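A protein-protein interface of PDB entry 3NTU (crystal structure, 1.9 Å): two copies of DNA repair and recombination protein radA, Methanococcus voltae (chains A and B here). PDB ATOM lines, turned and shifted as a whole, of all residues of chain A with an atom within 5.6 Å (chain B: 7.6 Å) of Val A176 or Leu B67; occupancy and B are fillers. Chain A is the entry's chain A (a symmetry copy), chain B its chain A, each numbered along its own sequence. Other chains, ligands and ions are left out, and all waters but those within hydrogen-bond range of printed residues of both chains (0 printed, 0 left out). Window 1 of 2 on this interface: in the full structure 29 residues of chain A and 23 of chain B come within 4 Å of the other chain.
The backbone carbonyl oxygen (O) of Lys B62 lies within hydrogen-bond range of the backbone NH (N) of Val A176, at 2.8 Å.
The backbone NH of Gly B64 sits at hydrogen-bond distance from the backbone carbonyl oxygen of Leu A171, 2.8 Å away.
The backbone carbonyl oxygen of Leu B68 lies within hydrogen-bond range of the side-chain hydroxyl of Ser B72, at 3.0 Å.
The backbone carbonyl oxygen (O) of Phe A175 is in hydrogen-bond range of the backbone NH (N) of Tyr A144, at 2.7 Å.
The backbone carbonyl oxygen (O) of Tyr A144 lies within hydrogen-bond range of the backbone NH (N) of Ala A177 (3.0 Å).
The backbone NH of Asp A146 is in hydrogen-bond range of the backbone carbonyl oxygen of Ala A177, at 2.9 Å.
Among the printed residues, merely in contact across the chains: Val A143 with Phe B61 (3.7 Å), Pro A153 with Leu B67 (3.6 Å), Pro A153 with Leu B68 (3.7 Å), Leu A171 with Ser B63 (3.9 Å), Leu A171 with Leu B67 (3.7 Å), Thr A174 with Lys B62 (3.7 Å), Thr A174 with Ser B63 (3.1 Å), Thr A174 with Leu B67 (3.8 Å), Phe A175 with Lys B62 (3.3 Å), Phe A175 with Ser B63 (3.98 Å), Val A176 with Gly B60 (3.7 Å), Val A176 with Phe B61 (3.6 Å), Val A176 with Leu B67 (3.5 Å), Ala A177 with Gly B60 (3.9 Å) and Ala A177 with Phe B61 (3.6 Å).
Val A176 touches four residues of chain B.
Printed residues of chain A within 4 Å of Leu B67: Pro A153, Leu A171, Thr A174 and Val A176.
Of the printed residues of chain A, Gly B64 touches Leu A171.
Of the printed residues of chain B, Thr A174 touches Lys B62, Ser B63 and Leu B67.
Of the printed residues of chain B, Pro A153 touches Leu B67 (3.6 Å) and Leu B68 (3.7 Å).
Printed residues of chain A within 4 Å of Gly B60: Val A176 (3.7 Å) and Ala A177 (3.9 Å).
The nearest residue of chain B that does not touch Val A176 is Ser B63 (5.0 Å).
The nearest residue of chain A that does not touch Leu B67 is Phe A151 (4.1 Å).
The nearest printed residue of chain B that does not touch Pro A153 is Arg B71 (4.03 Å).
Hydrophobic or aromatic side chains of chain B that line the printed part of chain A: Phe B61, Leu B67 and Leu B68.
Along chain B the printed residues that touch a printed residue of chain A span positions 60 to 68.
Among the printed residues, no Asp or Glu carboxylate lies within 4 Å of a Lys or Arg side-chain nitrogen of the other chain.
No position is printed for both chains.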
ATOM      1  N   VAL A 143      -0.347  17.164  -1.136  1.00  0.00           N
ATOM      2  CA  VAL A 143      -1.095  18.379  -1.468  1.00  0.00           C
ATOM      3  C   VAL A 143      -1.597  18.880  -0.086  1.00  0.00           C
ATOM      4  O   VAL A 143      -2.181  18.108   0.672  1.00  0.00           O
ATOM      5  CB  VAL A 143      -2.319  18.114  -2.366  1.00  0.00           C
ATOM      6  CG1 VAL A 143      -3.152  19.390  -2.492  1.00  0.00           C
ATOM      7  CG2 VAL A 143      -1.862  17.676  -3.751  1.00  0.00           C
ATOM      8  N   TYR A 144      -1.342  20.146   0.245  1.00  0.00           N
ATOM      9  CA  TYR A 144      -1.735  20.713   1.531  1.00  0.00           C
ATOM     10  C   TYR A 144      -2.669  21.895   1.223  1.00  0.00           C
ATOM     11  O   TYR A 144      -2.240  22.918   0.731  1.00  0.00           O
ATOM     12  CB  TYR A 144      -0.464  21.209   2.254  1.00  0.00           C
ATOM     13  CG  TYR A 144      -0.578  21.496   3.745  1.00  0.00           C
ATOM     14  CD1 TYR A 144       0.209  20.802   4.664  1.00  0.00           C
ATOM     15  CD2 TYR A 144      -1.472  22.444   4.224  1.00  0.00           C
ATOM     16  CE1 TYR A 144       0.102  21.040   6.037  1.00  0.00           C
ATOM     17  CE2 TYR A 144      -1.598  22.695   5.593  1.00  0.00           C
ATOM     18  CZ  TYR A 144      -0.802  21.981   6.491  1.00  0.00           C
ATOM     19  OH  TYR A 144      -0.964  22.183   7.832  1.00  0.00           O
ATOM     20  N   ILE A 145      -3.956  21.740   1.500  1.00  0.00           N
ATOM     21  CA  ILE A 145      -4.897  22.818   1.273  1.00  0.00           C
ATOM     22  C   ILE A 145      -5.021  23.530   2.632  1.00  0.00           C
ATOM     23  O   ILE A 145      -5.635  23.045   3.583  1.00  0.00           O
ATOM     24  CB  ILE A 145      -6.249  22.262   0.757  1.00  0.00           C
ATOM     25  CG1 ILE A 145      -6.020  21.705  -0.673  1.00  0.00           C
ATOM     26  CG2 ILE A 145      -7.304  23.402   0.727  1.00  0.00           C
ATOM     27  CD1 ILE A 145      -7.289  20.932  -1.283  1.00  0.00           C
ATOM     28  N   ASP A 146      -4.387  24.689   2.691  1.00  0.00           N
ATOM     29  CA  ASP A 146      -4.288  25.496   3.888  1.00  0.00           C
ATOM     30  C   ASP A 146      -5.397  26.530   3.906  1.00  0.00           C
ATOM     31  O   ASP A 146      -5.351  27.518   3.160  1.00  0.00           O
ATOM     32  CB  ASP A 146      -2.917  26.189   3.843  1.00  0.00           C
ATOM     33  CG  ASP A 146      -2.680  27.118   5.002  1.00  0.00           C
ATOM     34  OD1 ASP A 146      -3.482  27.109   5.960  1.00  0.00           O
ATOM     35  OD2 ASP A 146      -1.664  27.867   4.954  1.00  0.00           O
ATOM     36  N   PHE A 151       0.447  27.181   7.040  1.00  0.00           N
ATOM     37  CA  PHE A 151       1.493  26.298   6.504  1.00  0.00           C
ATOM     38  C   PHE A 151       2.822  27.030   6.830  1.00  0.00           C
ATOM     39  O   PHE A 151       2.923  28.244   6.627  1.00  0.00           O
ATOM     40  CB  PHE A 151       1.387  26.164   5.013  1.00  0.00           C
ATOM     41  CG  PHE A 151       2.431  25.269   4.446  1.00  0.00           C
ATOM     42  CD1 PHE A 151       2.331  23.896   4.625  1.00  0.00           C
ATOM     43  CD2 PHE A 151       3.544  25.795   3.793  1.00  0.00           C
ATOM     44  CE1 PHE A 151       3.334  23.030   4.167  1.00  0.00           C
ATOM     45  CE2 PHE A 151       4.555  24.941   3.331  1.00  0.00           C
ATOM     46  CZ  PHE A 151       4.444  23.569   3.520  1.00  0.00           C
ATOM     47  N   PRO A 153       6.838  26.704   5.971  1.00  0.00           N
ATOM     48  CA  PRO A 153       7.967  25.999   5.359  1.00  0.00           C
ATOM     49  C   PRO A 153       9.160  25.807   6.300  1.00  0.00           C
ATOM     50  O   PRO A 153       9.861  24.772   6.235  1.00  0.00           O
ATOM     51  CB  PRO A 153       8.270  26.823   4.094  1.00  0.00           C
ATOM     52  CG  PRO A 153       7.560  28.117   4.281  1.00  0.00           C
ATOM     53  CD  PRO A 153       6.380  27.841   5.153  1.00  0.00           C
ATOM     54  N   LEU A 171       9.793  20.294   0.419  1.00  0.00           N
ATOM     55  CA  LEU A 171       9.064  21.456  -0.130  1.00  0.00           C
ATOM     56  C   LEU A 171       8.862  21.282  -1.643  1.00  0.00           C
ATOM     57  O   LEU A 171       7.821  21.685  -2.221  1.00  0.00           O
ATOM     58  CB  LEU A 171       9.831  22.769   0.145  1.00  0.00           C
ATOM     59  CG  LEU A 171       9.998  23.166   1.601  1.00  0.00           C
ATOM     60  CD1 LEU A 171      10.874  24.436   1.696  1.00  0.00           C
ATOM     61  CD2 LEU A 171       8.631  23.455   2.226  1.00  0.00           C
ATOM     62  N   THR A 174       5.758  18.934  -2.276  1.00  0.00           N
ATOM     63  CA  THR A 174       4.526  19.282  -1.564  1.00  0.00           C
ATOM     64  C   THR A 174       3.896  20.485  -2.266  1.00  0.00           C
ATOM     65  O   THR A 174       4.546  21.516  -2.432  1.00  0.00           O
ATOM     66  CB  THR A 174       4.832  19.654  -0.106  1.00  0.00           C
ATOM     67  OG1 THR A 174       5.451  18.532   0.540  1.00  0.00           O
ATOM     68  CG2 THR A 174       3.521  20.064   0.655  1.00  0.00           C
ATOM     69  N   PHE A 175       2.644  20.351  -2.693  1.00  0.00           N
ATOM     70  CA  PHE A 175       1.916  21.454  -3.326  1.00  0.00           C
ATOM     71  C   PHE A 175       1.036  22.088  -2.244  1.00  0.00           C
ATOM     72  O   PHE A 175       0.278  21.379  -1.590  1.00  0.00           O
ATOM     73  CB  PHE A 175       0.985  20.951  -4.420  1.00  0.00           C
ATOM     74  CG  PHE A 175       1.690  20.370  -5.590  1.00  0.00           C
ATOM     75  CD1 PHE A 175       1.885  19.007  -5.684  1.00  0.00           C
ATOM     76  CD2 PHE A 175       2.188  21.205  -6.600  1.00  0.00           C
ATOM     77  CE1 PHE A 175       2.574  18.447  -6.763  1.00  0.00           C
ATOM     78  CE2 PHE A 175       2.880  20.650  -7.683  1.00  0.00           C
ATOM     79  CZ  PHE A 175       3.073  19.268  -7.760  1.00  0.00           C
ATOM     80  N   VAL A 176       1.107  23.399  -2.067  1.00  0.00           N
ATOM     81  CA  VAL A 176       0.278  24.060  -1.047  1.00  0.00           C
ATOM     82  C   VAL A 176      -0.669  25.049  -1.743  1.00  0.00           C
ATOM     83  O   VAL A 176      -0.248  25.803  -2.625  1.00  0.00           O
ATOM     84  CB  VAL A 176       1.138  24.853  -0.036  1.00  0.00           C
ATOM     85  CG1 VAL A 176       0.238  25.510   1.021  1.00  0.00           C
ATOM     86  CG2 VAL A 176       2.192  23.870   0.665  1.00  0.00           C
ATOM     87  N   ALA A 177      -1.946  25.010  -1.381  1.00  0.00           N
ATOM     88  CA  ALA A 177      -2.906  25.923  -1.984  1.00  0.00           C
ATOM     89  C   ALA A 177      -3.544  26.654  -0.807  1.00  0.00           C
ATOM     90  O   ALA A 177      -4.067  26.015   0.096  1.00  0.00           O
ATOM     91  CB  ALA A 177      -3.955  25.121  -2.747  1.00  0.00           C
ATOM     92  N   ARG A 178      -3.469  27.973  -0.791  1.00  0.00           N
ATOM     93  CA  ARG A 178      -4.092  28.764   0.281  1.00  0.00           C
ATOM     94  C   ARG A 178      -5.531  29.105  -0.149  1.00  0.00           C
ATOM     95  O   ARG A 178      -5.738  29.792  -1.160  1.00  0.00           O
ATOM     96  CB  ARG A 178      -3.321  30.081   0.504  1.00  0.00           C
ATOM     97  CG  ARG A 178      -3.981  31.039   1.490  1.00  0.00           C
ATOM     98  CD  ARG A 178      -3.625  30.707   2.948  1.00  0.00           C
ATOM     99  NE  ARG A 178      -4.193  31.728   3.822  1.00  0.00           N
ATOM    100  CZ  ARG A 178      -5.439  31.672   4.240  1.00  0.00           C
ATOM    101  NH1 ARG A 178      -6.162  30.648   3.874  1.00  0.00           N
ATOM    102  NH2 ARG A 178      -5.974  32.634   4.968  1.00  0.00           N
ATOM    103  N   LEU B  59      -3.641  32.616  -7.533  1.00  0.00           N
ATOM    104  CA  LEU B  59      -4.005  31.845  -6.350  1.00  0.00           C
ATOM    105  C   LEU B  59      -4.189  30.354  -6.639  1.00  0.00           C
ATOM    106  O   LEU B  59      -5.312  29.839  -6.548  1.00  0.00           O
ATOM    107  CB  LEU B  59      -5.302  32.393  -5.760  1.00  0.00           C
ATOM    108  CG  LEU B  59      -5.313  33.877  -5.418  1.00  0.00           C
ATOM    109  CD1 LEU B  59      -6.647  34.189  -4.774  1.00  0.00           C
ATOM    110  CD2 LEU B  59      -4.166  34.232  -4.482  1.00  0.00           C
ATOM    111  N   GLY B  60      -3.111  29.653  -6.972  1.00  0.00           N
ATOM    112  CA  GLY B  60      -3.230  28.226  -7.274  1.00  0.00           C
ATOM    113  C   GLY B  60      -2.290  27.390  -6.425  1.00  0.00           C
ATOM    114  O   GLY B  60      -1.919  27.795  -5.317  1.00  0.00           O
ATOM    115  N   PHE B  61      -1.913  26.214  -6.910  1.00  0.00           N
ATOM    116  CA  PHE B  61      -1.001  25.388  -6.144  1.00  0.00           C
ATOM    117  C   PHE B  61       0.408  25.932  -6.329  1.00  0.00           C
ATOM    118  O   PHE B  61       0.770  26.365  -7.432  1.00  0.00           O
ATOM    119  CB  PHE B  61      -1.002  23.943  -6.618  1.00  0.00           C
ATOM    120  CG  PHE B  61      -2.299  23.220  -6.376  1.00  0.00           C
ATOM    121  CD1 PHE B  61      -3.162  22.990  -7.421  1.00  0.00           C
ATOM    122  CD2 PHE B  61      -2.646  22.770  -5.099  1.00  0.00           C
ATOM    123  CE1 PHE B  61      -4.373  22.312  -7.216  1.00  0.00           C
ATOM    124  CE2 PHE B  61      -3.861  22.089  -4.879  1.00  0.00           C
ATOM    125  CZ  PHE B  61      -4.719  21.864  -5.950  1.00  0.00           C
ATOM    126  N   LYS B  62       1.193  25.932  -5.255  1.00  0.00           N
ATOM    127  CA  LYS B  62       2.579  26.365  -5.332  1.00  0.00           C
ATOM    128  C   LYS B  62       3.401  25.296  -4.662  1.00  0.00           C
ATOM    129  O   LYS B  62       2.889  24.553  -3.822  1.00  0.00           O
ATOM    130  CB  LYS B  62       2.785  27.706  -4.626  1.00  0.00           C
ATOM    131  CG  LYS B  62       2.004  28.840  -5.321  1.00  0.00           C
ATOM    132  CD  LYS B  62       2.097  30.158  -4.596  1.00  0.00           C
ATOM    133  CE  LYS B  62       1.101  31.161  -5.213  1.00  0.00           C
ATOM    134  NZ  LYS B  62       1.104  31.006  -6.696  1.00  0.00           N
ATOM    135  N   SER B  63       4.678  25.189  -5.041  1.00  0.00           N
ATOM    136  CA  SER B  63       5.543  24.216  -4.384  1.00  0.00           C
ATOM    137  C   SER B  63       6.970  24.720  -4.459  1.00  0.00           C
ATOM    138  O   SER B  63       7.238  25.762  -5.070  1.00  0.00           O
ATOM    139  CB  SER B  63       5.468  22.837  -5.053  1.00  0.00           C
ATOM    140  OG  SER B  63       5.888  22.913  -6.397  1.00  0.00           O
ATOM    141  N   GLY B  64       7.873  23.967  -3.846  1.00  0.00           N
ATOM    142  CA  GLY B  64       9.277  24.343  -3.882  1.00  0.00           C
ATOM    143  C   GLY B  64       9.588  25.714  -3.307  1.00  0.00           C
ATOM    144  O   GLY B  64       9.036  26.151  -2.284  1.00  0.00           O
ATOM    145  N   ILE B  65      10.475  26.437  -3.992  1.00  0.00           N
ATOM    146  CA  ILE B  65      10.912  27.743  -3.526  1.00  0.00           C
ATOM    147  C   ILE B  65       9.794  28.783  -3.402  1.00  0.00           C
ATOM    148  O   ILE B  65       9.885  29.717  -2.590  1.00  0.00           O
ATOM    149  CB  ILE B  65      12.056  28.272  -4.440  1.00  0.00           C
ATOM    150  CG1 ILE B  65      12.764  29.432  -3.756  1.00  0.00           C
ATOM    151  CG2 ILE B  65      11.484  28.715  -5.797  1.00  0.00           C
ATOM    152  CD1 ILE B  65      13.944  29.997  -4.569  1.00  0.00           C
ATOM    153  N   ASP B  66       8.730  28.627  -4.190  1.00  0.00           N
ATOM    154  CA  ASP B  66       7.607  29.548  -4.116  1.00  0.00           C
ATOM    155  C   ASP B  66       6.945  29.550  -2.738  1.00  0.00           C
ATOM    156  O   ASP B  66       6.317  30.531  -2.343  1.00  0.00           O
ATOM    157  CB  ASP B  66       6.554  29.198  -5.165  1.00  0.00           C
ATOM    158  CG  ASP B  66       7.047  29.390  -6.585  1.00  0.00           C
ATOM    159  OD1 ASP B  66       6.223  29.196  -7.509  1.00  0.00           O
ATOM    160  OD2 ASP B  66       8.246  29.731  -6.783  1.00  0.00           O
ATOM    161  N   LEU B  67       7.061  28.444  -2.016  1.00  0.00           N
ATOM    162  CA  LEU B  67       6.461  28.349  -0.671  1.00  0.00           C
ATOM    163  C   LEU B  67       7.207  29.283   0.279  1.00  0.00           C
ATOM    164  O   LEU B  67       6.633  29.856   1.221  1.00  0.00           O
ATOM    165  CB  LEU B  67       6.515  26.890  -0.168  1.00  0.00           C
ATOM    166  CG  LEU B  67       5.771  25.839  -1.018  1.00  0.00           C
ATOM    167  CD1 LEU B  67       5.973  24.411  -0.466  1.00  0.00           C
ATOM    168  CD2 LEU B  67       4.287  26.172  -1.028  1.00  0.00           C
ATOM    169  N   LEU B  68       8.506  29.463   0.030  1.00  0.00           N
ATOM    170  CA  LEU B  68       9.301  30.355   0.870  1.00  0.00           C
ATOM    171  C   LEU B  68       8.955  31.822   0.594  1.00  0.00           C
ATOM    172  O   LEU B  68       8.968  32.666   1.507  1.00  0.00           O
ATOM    173  CB  LEU B  68      10.804  30.111   0.623  1.00  0.00           C
ATOM    174  CG  LEU B  68      11.313  28.703   0.957  1.00  0.00           C
ATOM    175  CD1 LEU B  68      12.804  28.567   0.557  1.00  0.00           C
ATOM    176  CD2 LEU B  68      11.189  28.458   2.445  1.00  0.00           C
ATOM    177  N   LYS B  69       8.618  32.123  -0.653  1.00  0.00           N
ATOM    178  CA  LYS B  69       8.303  33.497  -1.048  1.00  0.00           C
ATOM    179  C   LYS B  69       7.024  34.003  -0.391  1.00  0.00           C
ATOM    180  O   LYS B  69       6.901  35.181  -0.048  1.00  0.00           O
ATOM    181  CB  LYS B  69       8.206  33.610  -2.575  1.00  0.00           C
ATOM    182  CG  LYS B  69       9.551  33.320  -3.282  1.00  0.00           C
ATOM    183  CD  LYS B  69       9.463  33.558  -4.792  1.00  0.00           C
ATOM    184  CE  LYS B  69      10.824  33.389  -5.470  1.00  0.00           C
ATOM    185  NZ  LYS B  69      11.385  32.036  -5.193  1.00  0.00           N
ATOM    186  N   GLN B  70       6.073  33.108  -0.198  1.00  0.00           N
ATOM    187  CA  GLN B  70       4.853  33.526   0.437  1.00  0.00           C
ATOM    188  C   GLN B  70       5.134  33.911   1.901  1.00  0.00           C
ATOM    189  O   GLN B  70       4.645  34.912   2.409  1.00  0.00           O
ATOM    190  CB  GLN B  70       3.839  32.395   0.360  1.00  0.00           C
ATOM    191  CG  GLN B  70       2.566  32.670   1.124  1.00  0.00           C
ATOM    192  CD  GLN B  70       1.844  33.958   0.673  1.00  0.00           C
ATOM    193  OE1 GLN B  70       1.428  34.775   1.511  1.00  0.00           O
ATOM    194  NE2 GLN B  70       1.681  34.126  -0.641  1.00  0.00           N
ATOM    195  N   ARG B  71       5.918  33.089   2.577  1.00  0.00           N
ATOM    196  CA  ARG B  71       6.232  33.329   3.963  1.00  0.00           C
ATOM    197  C   ARG B  71       7.034  34.632   4.079  1.00  0.00           C
ATOM    198  O   ARG B  71       6.895  35.361   5.054  1.00  0.00           O
ATOM    199  CB  ARG B  71       6.973  32.094   4.514  1.00  0.00           C
ATOM    200  CG  ARG B  71       7.252  32.065   6.001  1.00  0.00           C
ATOM    201  CD  ARG B  71       5.974  32.127   6.916  1.00  0.00           C
ATOM    202  NE  ARG B  71       6.444  32.213   8.298  1.00  0.00           N
ATOM    203  CZ  ARG B  71       5.844  32.891   9.280  1.00  0.00           C
ATOM    204  NH1 ARG B  71       4.719  33.551   9.053  1.00  0.00           N
ATOM    205  NH2 ARG B  71       6.414  32.927  10.477  1.00  0.00           N
ATOM    206  N   SER B  72       7.819  34.967   3.053  1.00  0.00           N
ATOM    207  CA  SER B  72       8.612  36.203   3.090  1.00  0.00           C
ATOM    208  C   SER B  72       7.815  37.492   2.973  1.00  0.00           C
ATOM    209  O   SER B  72       8.377  38.577   3.153  1.00  0.00           O
ATOM    210  CB  SER B  72       9.688  36.176   1.998  1.00  0.00           C
ATOM    211  OG  SER B  72      10.551  35.079   2.248  1.00  0.00           O
